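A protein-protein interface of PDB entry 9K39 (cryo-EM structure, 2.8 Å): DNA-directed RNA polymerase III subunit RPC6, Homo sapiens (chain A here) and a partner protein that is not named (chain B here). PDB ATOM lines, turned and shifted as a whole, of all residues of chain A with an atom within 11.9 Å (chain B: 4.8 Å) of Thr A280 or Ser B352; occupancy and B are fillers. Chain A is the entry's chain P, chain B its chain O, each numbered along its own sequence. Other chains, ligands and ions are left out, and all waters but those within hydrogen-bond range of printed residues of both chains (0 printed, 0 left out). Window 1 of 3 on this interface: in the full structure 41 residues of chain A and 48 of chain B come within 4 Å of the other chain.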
ATOM      1  N   ILE A 243      19.877  31.432 -11.228  1.00  0.00           N
ATOM      2  CA  ILE A 243      19.726  32.676 -10.477  1.00  0.00           C
ATOM      3  C   ILE A 243      18.957  32.418  -9.189  1.00  0.00           C
ATOM      4  O   ILE A 243      19.332  32.896  -8.112  1.00  0.00           O
ATOM      5  CB  ILE A 243      19.027  33.744 -11.338  1.00  0.00           C
ATOM      6  CG1 ILE A 243      19.898  34.134 -12.532  1.00  0.00           C
ATOM      7  CG2 ILE A 243      18.693  34.972 -10.503  1.00  0.00           C
ATOM      8  CD1 ILE A 243      19.143  34.895 -13.594  1.00  0.00           C
ATOM      9  N   TYR A 244      17.866  31.658  -9.287  1.00  0.00           N
ATOM     10  CA  TYR A 244      17.087  31.306  -8.108  1.00  0.00           C
ATOM     11  C   TYR A 244      17.883  30.466  -7.116  1.00  0.00           C
ATOM     12  O   TYR A 244      17.491  30.375  -5.952  1.00  0.00           O
ATOM     13  CB  TYR A 244      15.814  30.564  -8.522  1.00  0.00           C
ATOM     14  CG  TYR A 244      14.903  31.363  -9.427  1.00  0.00           C
ATOM     15  CD1 TYR A 244      14.815  32.745  -9.310  1.00  0.00           C
ATOM     16  CD2 TYR A 244      14.141  30.738 -10.404  1.00  0.00           C
ATOM     17  CE1 TYR A 244      13.985  33.480 -10.136  1.00  0.00           C
ATOM     18  CE2 TYR A 244      13.312  31.467 -11.237  1.00  0.00           C
ATOM     19  CZ  TYR A 244      13.238  32.835 -11.098  1.00  0.00           C
ATOM     20  OH  TYR A 244      12.411  33.564 -11.923  1.00  0.00           O
ATOM     21  N   ASP A 245      18.983  29.856  -7.551  1.00  0.00           N
ATOM     22  CA  ASP A 245      19.855  29.114  -6.649  1.00  0.00           C
ATOM     23  C   ASP A 245      20.832  30.014  -5.903  1.00  0.00           C
ATOM     24  O   ASP A 245      21.572  29.521  -5.046  1.00  0.00           O
ATOM     25  CB  ASP A 245      20.624  28.041  -7.427  1.00  0.00           C
ATOM     26  CG  ASP A 245      21.054  26.878  -6.552  1.00  0.00           C
ATOM     27  OD1 ASP A 245      20.704  26.869  -5.354  1.00  0.00           O
ATOM     28  OD2 ASP A 245      21.740  25.972  -7.066  1.00  0.00           O
ATOM     29  N   GLY A 246      20.851  31.310  -6.202  1.00  0.00           N
ATOM     30  CA  GLY A 246      21.747  32.225  -5.523  1.00  0.00           C
ATOM     31  C   GLY A 246      23.193  32.142  -5.945  1.00  0.00           C
ATOM     32  O   GLY A 246      24.080  32.434  -5.137  1.00  0.00           O
ATOM     33  N   LYS A 247      23.464  31.749  -7.191  1.00  0.00           N
ATOM     34  CA  LYS A 247      24.829  31.537  -7.653  1.00  0.00           C
ATOM     35  C   LYS A 247      25.241  32.436  -8.811  1.00  0.00           C
ATOM     36  O   LYS A 247      26.442  32.647  -9.001  1.00  0.00           O
ATOM     37  CB  LYS A 247      25.021  30.071  -8.065  1.00  0.00           C
ATOM     38  CG  LYS A 247      24.695  29.081  -6.955  1.00  0.00           C
ATOM     39  CD  LYS A 247      24.507  27.671  -7.494  1.00  0.00           C
ATOM     40  CE  LYS A 247      25.789  27.128  -8.099  1.00  0.00           C
ATOM     41  NZ  LYS A 247      25.597  25.760  -8.657  1.00  0.00           N
ATOM     42  N   ASN A 274      29.816  35.353  -6.465  1.00  0.00           N
ATOM     43  CA  ASN A 274      29.971  34.676  -5.188  1.00  0.00           C
ATOM     44  C   ASN A 274      28.820  35.045  -4.252  1.00  0.00           C
ATOM     45  O   ASN A 274      28.195  36.098  -4.407  1.00  0.00           O
ATOM     46  CB  ASN A 274      31.305  35.053  -4.548  1.00  0.00           C
ATOM     47  CG  ASN A 274      32.493  34.683  -5.416  1.00  0.00           C
ATOM     48  OD1 ASN A 274      32.441  33.722  -6.182  1.00  0.00           O
ATOM     49  ND2 ASN A 274      33.572  35.448  -5.299  1.00  0.00           N
ATOM     50  N   PRO A 275      28.511  34.189  -3.278  1.00  0.00           N
ATOM     51  CA  PRO A 275      27.441  34.515  -2.328  1.00  0.00           C
ATOM     52  C   PRO A 275      27.791  35.727  -1.479  1.00  0.00           C
ATOM     53  O   PRO A 275      28.954  36.112  -1.348  1.00  0.00           O
ATOM     54  CB  PRO A 275      27.328  33.248  -1.469  1.00  0.00           C
ATOM     55  CG  PRO A 275      28.644  32.559  -1.629  1.00  0.00           C
ATOM     56  CD  PRO A 275      29.076  32.850  -3.032  1.00  0.00           C
ATOM     57  N   ILE A 276      26.751  36.334  -0.904  1.00  0.00           N
ATOM     58  CA  ILE A 276      26.936  37.556  -0.121  1.00  0.00           C
ATOM     59  C   ILE A 276      27.744  37.267   1.137  1.00  0.00           C
ATOM     60  O   ILE A 276      28.788  37.887   1.385  1.00  0.00           O
ATOM     61  CB  ILE A 276      25.574  38.187   0.219  1.00  0.00           C
ATOM     62  CG1 ILE A 276      24.798  38.504  -1.060  1.00  0.00           C
ATOM     63  CG2 ILE A 276      25.763  39.440   1.057  1.00  0.00           C
ATOM     64  CD1 ILE A 276      23.439  39.124  -0.812  1.00  0.00           C
ATOM     65  N   ILE A 277      27.283  36.321   1.948  1.00  0.00           N
ATOM     66  CA  ILE A 277      27.931  36.004   3.219  1.00  0.00           C
ATOM     67  C   ILE A 277      28.100  34.499   3.335  1.00  0.00           C
ATOM     68  O   ILE A 277      27.330  33.721   2.760  1.00  0.00           O
ATOM     69  CB  ILE A 277      27.132  36.540   4.425  1.00  0.00           C
ATOM     70  CG1 ILE A 277      25.699  36.006   4.397  1.00  0.00           C
ATOM     71  CG2 ILE A 277      27.143  38.062   4.445  1.00  0.00           C
ATOM     72  CD1 ILE A 277      24.855  36.462   5.565  1.00  0.00           C
ATOM     73  N   PRO A 278      29.116  34.060   4.075  1.00  0.00           N
ATOM     74  CA  PRO A 278      29.285  32.625   4.338  1.00  0.00           C
ATOM     75  C   PRO A 278      28.127  32.087   5.160  1.00  0.00           C
ATOM     76  O   PRO A 278      27.290  32.867   5.644  1.00  0.00           O
ATOM     77  CB  PRO A 278      30.604  32.566   5.127  1.00  0.00           C
ATOM     78  CG  PRO A 278      31.328  33.811   4.744  1.00  0.00           C
ATOM     79  CD  PRO A 278      30.261  34.847   4.565  1.00  0.00           C
ATOM     80  N   PRO A 279      28.024  30.767   5.323  1.00  0.00           N
ATOM     81  CA  PRO A 279      26.958  30.211   6.164  1.00  0.00           C
ATOM     82  C   PRO A 279      26.974  30.812   7.563  1.00  0.00           C
ATOM     83  O   PRO A 279      28.030  30.975   8.180  1.00  0.00           O
ATOM     84  CB  PRO A 279      27.272  28.712   6.189  1.00  0.00           C
ATOM     85  CG  PRO A 279      27.957  28.468   4.891  1.00  0.00           C
ATOM     86  CD  PRO A 279      28.771  29.708   4.617  1.00  0.00           C
ATOM     87  N   THR A 280      25.785  31.143   8.058  1.00  0.00           N
ATOM     88  CA  THR A 280      25.653  31.836   9.329  1.00  0.00           C
ATOM     89  C   THR A 280      26.001  30.905  10.492  1.00  0.00           C
ATOM     90  O   THR A 280      26.146  29.688  10.338  1.00  0.00           O
ATOM     91  CB  THR A 280      24.237  32.382   9.494  1.00  0.00           C
ATOM     92  OG1 THR A 280      23.298  31.300   9.492  1.00  0.00           O
ATOM     93  CG2 THR A 280      23.904  33.334   8.355  1.00  0.00           C
ATOM     94  N   GLY A 281      26.139  31.504  11.676  1.00  0.00           N
ATOM     95  CA  GLY A 281      26.484  30.742  12.863  1.00  0.00           C
ATOM     96  C   GLY A 281      25.363  29.874  13.396  1.00  0.00           C
ATOM     97  O   GLY A 281      25.634  28.902  14.109  1.00  0.00           O
ATOM     98  N   LEU A 282      24.110  30.200  13.068  1.00  0.00           N
ATOM     99  CA  LEU A 282      22.986  29.413  13.564  1.00  0.00           C
ATOM    100  C   LEU A 282      23.016  27.994  13.012  1.00  0.00           C
ATOM    101  O   LEU A 282      22.772  27.029  13.744  1.00  0.00           O
ATOM    102  CB  LEU A 282      21.666  30.095  13.208  1.00  0.00           C
ATOM    103  CG  LEU A 282      20.408  29.279  13.528  1.00  0.00           C
ATOM    104  CD1 LEU A 282      20.252  29.089  15.031  1.00  0.00           C
ATOM    105  CD2 LEU A 282      19.171  29.931  12.932  1.00  0.00           C
ATOM    106  N   VAL A 283      23.315  27.848  11.718  1.00  0.00           N
ATOM    107  CA  VAL A 283      23.336  26.529  11.095  1.00  0.00           C
ATOM    108  C   VAL A 283      24.515  25.686  11.549  1.00  0.00           C
ATOM    109  O   VAL A 283      24.530  24.475  11.303  1.00  0.00           O
ATOM    110  CB  VAL A 283      23.351  26.660   9.559  1.00  0.00           C
ATOM    111  CG1 VAL A 283      22.280  27.636   9.106  1.00  0.00           C
ATOM    112  CG2 VAL A 283      24.722  27.097   9.071  1.00  0.00           C
ATOM    113  N   ARG A 284      25.505  26.294  12.203  1.00  0.00           N
ATOM    114  CA  ARG A 284      26.637  25.548  12.734  1.00  0.00           C
ATOM    115  C   ARG A 284      26.328  24.880  14.066  1.00  0.00           C
ATOM    116  O   ARG A 284      27.184  24.159  14.591  1.00  0.00           O
ATOM    117  CB  ARG A 284      27.849  26.469  12.883  1.00  0.00           C
ATOM    118  CG  ARG A 284      28.365  27.024  11.563  1.00  0.00           C
ATOM    119  CD  ARG A 284      29.667  27.780  11.749  1.00  0.00           C
ATOM    120  NE  ARG A 284      30.251  28.189  10.476  1.00  0.00           N
ATOM    121  CZ  ARG A 284      30.014  29.355   9.883  1.00  0.00           C
ATOM    122  NH1 ARG A 284      29.199  30.235  10.449  1.00  0.00           N
ATOM    123  NH2 ARG A 284      30.590  29.641   8.724  1.00  0.00           N
ATOM    124  N   ALA A 285      25.136  25.099  14.621  1.00  0.00           N
ATOM    125  CA  ALA A 285      24.700  24.470  15.853  1.00  0.00           C
ATOM    126  C   ALA A 285      23.575  23.481  15.570  1.00  0.00           C
ATOM    127  O   ALA A 285      22.737  23.732  14.698  1.00  0.00           O
ATOM    128  CB  ALA A 285      24.215  25.510  16.869  1.00  0.00           C
ATOM    129  N   PRO A 286      23.537  22.347  16.277  1.00  0.00           N
ATOM    130  CA  PRO A 286      22.462  21.370  16.031  1.00  0.00           C
ATOM    131  C   PRO A 286      21.075  21.910  16.324  1.00  0.00           C
ATOM    132  O   PRO A 286      20.093  21.411  15.759  1.00  0.00           O
ATOM    133  CB  PRO A 286      22.826  20.209  16.966  1.00  0.00           C
ATOM    134  CG  PRO A 286      24.291  20.366  17.223  1.00  0.00           C
ATOM    135  CD  PRO A 286      24.536  21.844  17.233  1.00  0.00           C
ATOM    136  N   CYS A 287      20.960  22.915  17.196  1.00  0.00           N
ATOM    137  CA  CYS A 287      19.649  23.455  17.540  1.00  0.00           C
ATOM    138  C   CYS A 287      19.007  24.176  16.361  1.00  0.00           C
ATOM    139  O   CYS A 287      17.778  24.182  16.233  1.00  0.00           O
ATOM    140  CB  CYS A 287      19.769  24.403  18.733  1.00  0.00           C
ATOM    141  SG  CYS A 287      20.888  23.833  20.036  1.00  0.00           S
ATOM    142  N   GLY A 288      19.818  24.785  15.494  1.00  0.00           N
ATOM    143  CA  GLY A 288      19.281  25.525  14.365  1.00  0.00           C
ATOM    144  C   GLY A 288      18.760  24.652  13.242  1.00  0.00           C
ATOM    145  O   GLY A 288      17.920  25.107  12.459  1.00  0.00           O
ATOM    146  N   LEU A 289      19.239  23.414  13.148  1.00  0.00           N
ATOM    147  CA  LEU A 289      18.810  22.483  12.113  1.00  0.00           C
ATOM    148  C   LEU A 289      17.951  21.353  12.668  1.00  0.00           C
ATOM    149  O   LEU A 289      17.738  20.350  11.979  1.00  0.00           O
ATOM    150  CB  LEU A 289      20.025  21.909  11.383  1.00  0.00           C
ATOM    151  CG  LEU A 289      21.032  22.927  10.841  1.00  0.00           C
ATOM    152  CD1 LEU A 289      22.156  22.229  10.092  1.00  0.00           C
ATOM    153  CD2 LEU A 289      20.345  23.950   9.950  1.00  0.00           C
ATOM    154  N   TRP A 313      27.164  15.478  17.419  1.00  0.00           N
ATOM    155  CA  TRP A 313      27.910  16.625  16.914  1.00  0.00           C
ATOM    156  C   TRP A 313      29.198  16.845  17.702  1.00  0.00           C
ATOM    157  O   TRP A 313      30.242  17.154  17.114  1.00  0.00           O
ATOM    158  CB  TRP A 313      27.019  17.865  16.953  1.00  0.00           C
ATOM    159  CG  TRP A 313      27.721  19.152  16.672  1.00  0.00           C
ATOM    160  CD1 TRP A 313      28.323  19.524  15.504  1.00  0.00           C
ATOM    161  CD2 TRP A 313      27.873  20.256  17.568  1.00  0.00           C
ATOM    162  NE1 TRP A 313      28.852  20.786  15.627  1.00  0.00           N
ATOM    163  CE2 TRP A 313      28.588  21.257  16.885  1.00  0.00           C
ATOM    164  CE3 TRP A 313      27.478  20.491  18.890  1.00  0.00           C
ATOM    165  CZ2 TRP A 313      28.914  22.474  17.476  1.00  0.00           C
ATOM    166  CZ3 TRP A 313      27.804  21.698  19.475  1.00  0.00           C
ATOM    167  CH2 TRP A 313      28.516  22.675  18.768  1.00  0.00           C
ATOM    168  N   ALA B 348      20.299  37.404   2.991  1.00  0.00           N
ATOM    169  CA  ALA B 348      21.349  36.408   2.808  1.00  0.00           C
ATOM    170  C   ALA B 348      21.374  35.412   3.961  1.00  0.00           C
ATOM    171  O   ALA B 348      21.508  34.204   3.744  1.00  0.00           O
ATOM    172  CB  ALA B 348      22.706  37.098   2.663  1.00  0.00           C
ATOM    173  N   THR B 349      21.234  35.903   5.196  1.00  0.00           N
ATOM    174  CA  THR B 349      21.190  35.011   6.351  1.00  0.00           C
ATOM    175  C   THR B 349      20.008  34.051   6.262  1.00  0.00           C
ATOM    176  O   THR B 349      20.147  32.849   6.530  1.00  0.00           O
ATOM    177  CB  THR B 349      21.120  35.831   7.640  1.00  0.00           C
ATOM    178  OG1 THR B 349      22.371  36.499   7.853  1.00  0.00           O
ATOM    179  CG2 THR B 349      20.809  34.941   8.834  1.00  0.00           C
ATOM    180  N   LEU B 350      18.837  34.563   5.875  1.00  0.00           N
ATOM    181  CA  LEU B 350      17.649  33.719   5.805  1.00  0.00           C
ATOM    182  C   LEU B 350      17.778  32.672   4.702  1.00  0.00           C
ATOM    183  O   LEU B 350      17.448  31.498   4.910  1.00  0.00           O
ATOM    184  CB  LEU B 350      16.406  34.582   5.591  1.00  0.00           C
ATOM    185  CG  LEU B 350      15.055  33.897   5.782  1.00  0.00           C
ATOM    186  CD1 LEU B 350      14.996  33.189   7.125  1.00  0.00           C
ATOM    187  CD2 LEU B 350      13.929  34.914   5.665  1.00  0.00           C
ATOM    188  N   GLU B 351      18.268  33.070   3.526  1.00  0.00           N
ATOM    189  CA  GLU B 351      18.429  32.098   2.452  1.00  0.00           C
ATOM    190  C   GLU B 351      19.500  31.071   2.800  1.00  0.00           C
ATOM    191  O   GLU B 351      19.374  29.894   2.451  1.00  0.00           O
ATOM    192  CB  GLU B 351      18.745  32.802   1.129  1.00  0.00           C
ATOM    193  CG  GLU B 351      20.112  33.459   1.055  1.00  0.00           C
ATOM    194  CD  GLU B 351      20.359  34.141  -0.274  1.00  0.00           C
ATOM    195  OE1 GLU B 351      19.414  34.223  -1.088  1.00  0.00           O
ATOM    196  OE2 GLU B 351      21.498  34.598  -0.507  1.00  0.00           O
ATOM    197  N   SER B 352      20.540  31.485   3.531  1.00  0.00           N
ATOM    198  CA  SER B 352      21.580  30.545   3.932  1.00  0.00           C
ATOM    199  C   SER B 352      21.052  29.530   4.937  1.00  0.00           C
ATOM    200  O   SER B 352      21.347  28.333   4.830  1.00  0.00           O
ATOM    201  CB  SER B 352      22.776  31.302   4.510  1.00  0.00           C
ATOM    202  OG  SER B 352      23.795  30.408   4.920  1.00  0.00           O
ATOM    203  N   VAL B 353      20.267  29.981   5.921  1.00  0.00           N
ATOM    204  CA  VAL B 353      19.738  29.039   6.903  1.00  0.00           C
ATOM    205  C   VAL B 353      18.709  28.115   6.253  1.00  0.00           C
ATOM    206  O   VAL B 353      18.639  26.925   6.578  1.00  0.00           O
ATOM    207  CB  VAL B 353      19.167  29.779   8.130  1.00  0.00           C
ATOM    208  CG1 VAL B 353      17.954  30.613   7.772  1.00  0.00           C
ATOM    209  CG2 VAL B 353      18.821  28.787   9.234  1.00  0.00           C
ATOM    210  N   VAL B 354      17.934  28.627   5.292  1.00  0.00           N
ATOM    211  CA  VAL B 354      17.003  27.770   4.563  1.00  0.00           C
ATOM    212  C   VAL B 354      17.762  26.714   3.766  1.00  0.00           C
ATOM    213  O   VAL B 354      17.390  25.534   3.758  1.00  0.00           O
ATOM    214  CB  VAL B 354      16.085  28.617   3.660  1.00  0.00           C
ATOM    215  CG1 VAL B 354      15.354  27.733   2.659  1.00  0.00           C
ATOM    216  CG2 VAL B 354      15.090  29.396   4.503  1.00  0.00           C
ATOM    217  N   GLN B 355      18.840  27.120   3.088  1.00  0.00           N
ATOM    218  CA  GLN B 355      19.630  26.175   2.309  1.00  0.00           C
ATOM    219  C   GLN B 355      20.257  25.110   3.195  1.00  0.00           C
ATOM    220  O   GLN B 355      20.271  23.923   2.841  1.00  0.00           O
ATOM    221  CB  GLN B 355      20.712  26.918   1.525  1.00  0.00           C
ATOM    222  CG  GLN B 355      21.557  26.027   0.630  1.00  0.00           C
ATOM    223  CD  GLN B 355      22.589  26.807  -0.163  1.00  0.00           C
ATOM    224  OE1 GLN B 355      22.627  28.035  -0.116  1.00  0.00           O
ATOM    225  NE2 GLN B 355      23.432  26.090  -0.898  1.00  0.00           N
ATOM    226  N   GLU B 356      20.785  25.508   4.354  1.00  0.00           N
ATOM    227  CA  GLU B 356      21.438  24.548   5.234  1.00  0.00           C
ATOM    228  C   GLU B 356      20.447  23.685   6.005  1.00  0.00           C
ATOM    229  O   GLU B 356      20.834  22.624   6.507  1.00  0.00           O
ATOM    230  CB  GLU B 356      22.370  25.274   6.205  1.00  0.00           C
ATOM    231  CG  GLU B 356      23.574  25.923   5.544  1.00  0.00           C
ATOM    232  CD  GLU B 356      24.551  24.909   4.975  1.00  0.00           C
ATOM    233  OE1 GLU B 356      24.535  23.743   5.424  1.00  0.00           O
ATOM    234  OE2 GLU B 356      25.336  25.278   4.075  1.00  0.00           O
ATOM    235  N   GLU B 518      26.838  36.188  16.062  1.00  0.00           N
ATOM    236  CA  GLU B 518      26.930  37.023  14.868  1.00  0.00           C
ATOM    237  C   GLU B 518      25.591  37.087  14.136  1.00  0.00           C
ATOM    238  O   GLU B 518      25.128  38.170  13.752  1.00  0.00           O
ATOM    239  CB  GLU B 518      28.032  36.493  13.945  1.00  0.00           C
ATOM    240  CG  GLU B 518      28.128  37.194  12.597  1.00  0.00           C
ATOM    241  CD  GLU B 518      27.327  36.498  11.513  1.00  0.00           C
ATOM    242  OE1 GLU B 518      26.744  35.429  11.794  1.00  0.00           O
ATOM    243  OE2 GLU B 518      27.280  37.019  10.379  1.00  0.00           O
ATOM    244  N   THR B 519      24.960  35.928  13.929  1.00  0.00           N
ATOM    245  CA  THR B 519      23.630  35.906  13.329  1.00  0.00           C
ATOM    246  C   THR B 519      22.626  36.642  14.207  1.00  0.00           C
ATOM    247  O   THR B 519      21.733  37.336  13.699  1.00  0.00           O
ATOM    248  CB  THR B 519      23.184  34.461  13.099  1.00  0.00           C
ATOM    249  OG1 THR B 519      24.178  33.770  12.334  1.00  0.00           O
ATOM    250  CG2 THR B 519      21.859  34.424  12.350  1.00  0.00           C
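N of Gly A281 is in hydrogen-bond range of OG1 of Thr B519 (3.1 Å).
OE1 of Glu B518 sits at hydrogen-bond distance from OG1 of Thr B519 (3.1 Å).
O of Pro A279 is in hydrogen-bond range of NH1 of Arg A284, 2.7 Å away.
O of Thr A280 lies within hydrogen-bond range of NH1 of Arg A284.
Among the printed residues, pairs that only touch across the chains: Ile A276 with Ala B348, Ile A277 with Ala B348, Ile A277 with Thr B349, Pro A279 with Ser B352, Thr A280 with Thr B349, Thr A280 with Ser B352, Thr A280 with Thr B519, Gly A281 with Glu B518, Leu A282 with Val B353, Leu A282 with Thr B519, Val A283 with Val B353, Val A283 with Glu B356 and Leu A289 with Glu B356.
Tyr A244 touches none of the printed residues of chain B.
Of the printed residues of chain B, Ile A276 touches Ala B348 (3.9 Å).
Of the printed residues of chain B, Ile A277 touches Ala B348 (3.6 Å) and Thr B349 (3.4 Å).
Of the printed residues of chain B, Gly A281 touches Glu B518 (3.97 Å) and Thr B519 (3.1 Å).
Printed residues of chain B within 4 Å of Leu A282: Val B353 and Thr B519.
Printed residues of chain B within 4 Å of Val A283: Val B353 and Glu B356.
Thr B349 touches two residues of chain A.
No residue of chain A comes within 4 Å of Glu B351.
Ser B352 touches just these residues of chain A: Pro A279 and Thr A280.
Of chain A, only Leu A282 (3.9 Å) and Val A283 (3.6 Å) come within 4 Å of Val B353.
No residue of chain A comes within 4 Å of Gln B355.
Of chain A, only Val A283 and Leu A289 come within 4 Å of Glu B356.
Glu B518 touches just one residue of chain A: Gly A281 (3.97 Å).
Of the printed residues of chain A, Thr B519 touches Thr A280, Gly A281 and Leu A282.
The nearest residue of chain B that does not touch Thr A280 is Glu B518 (4.5 Å).
Printed residues of chain A that touch a printed residue of chain B: Ile A276, Ile A277, Pro A279, Thr A280, Gly A281, Leu A282, Val A283 and Leu A289.
Hydrophobic or aromatic side chains of chain A within 4 Å of the printed part of chain B: Ile A276, Ile A277, Leu A282, Val A283 and Leu A289.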
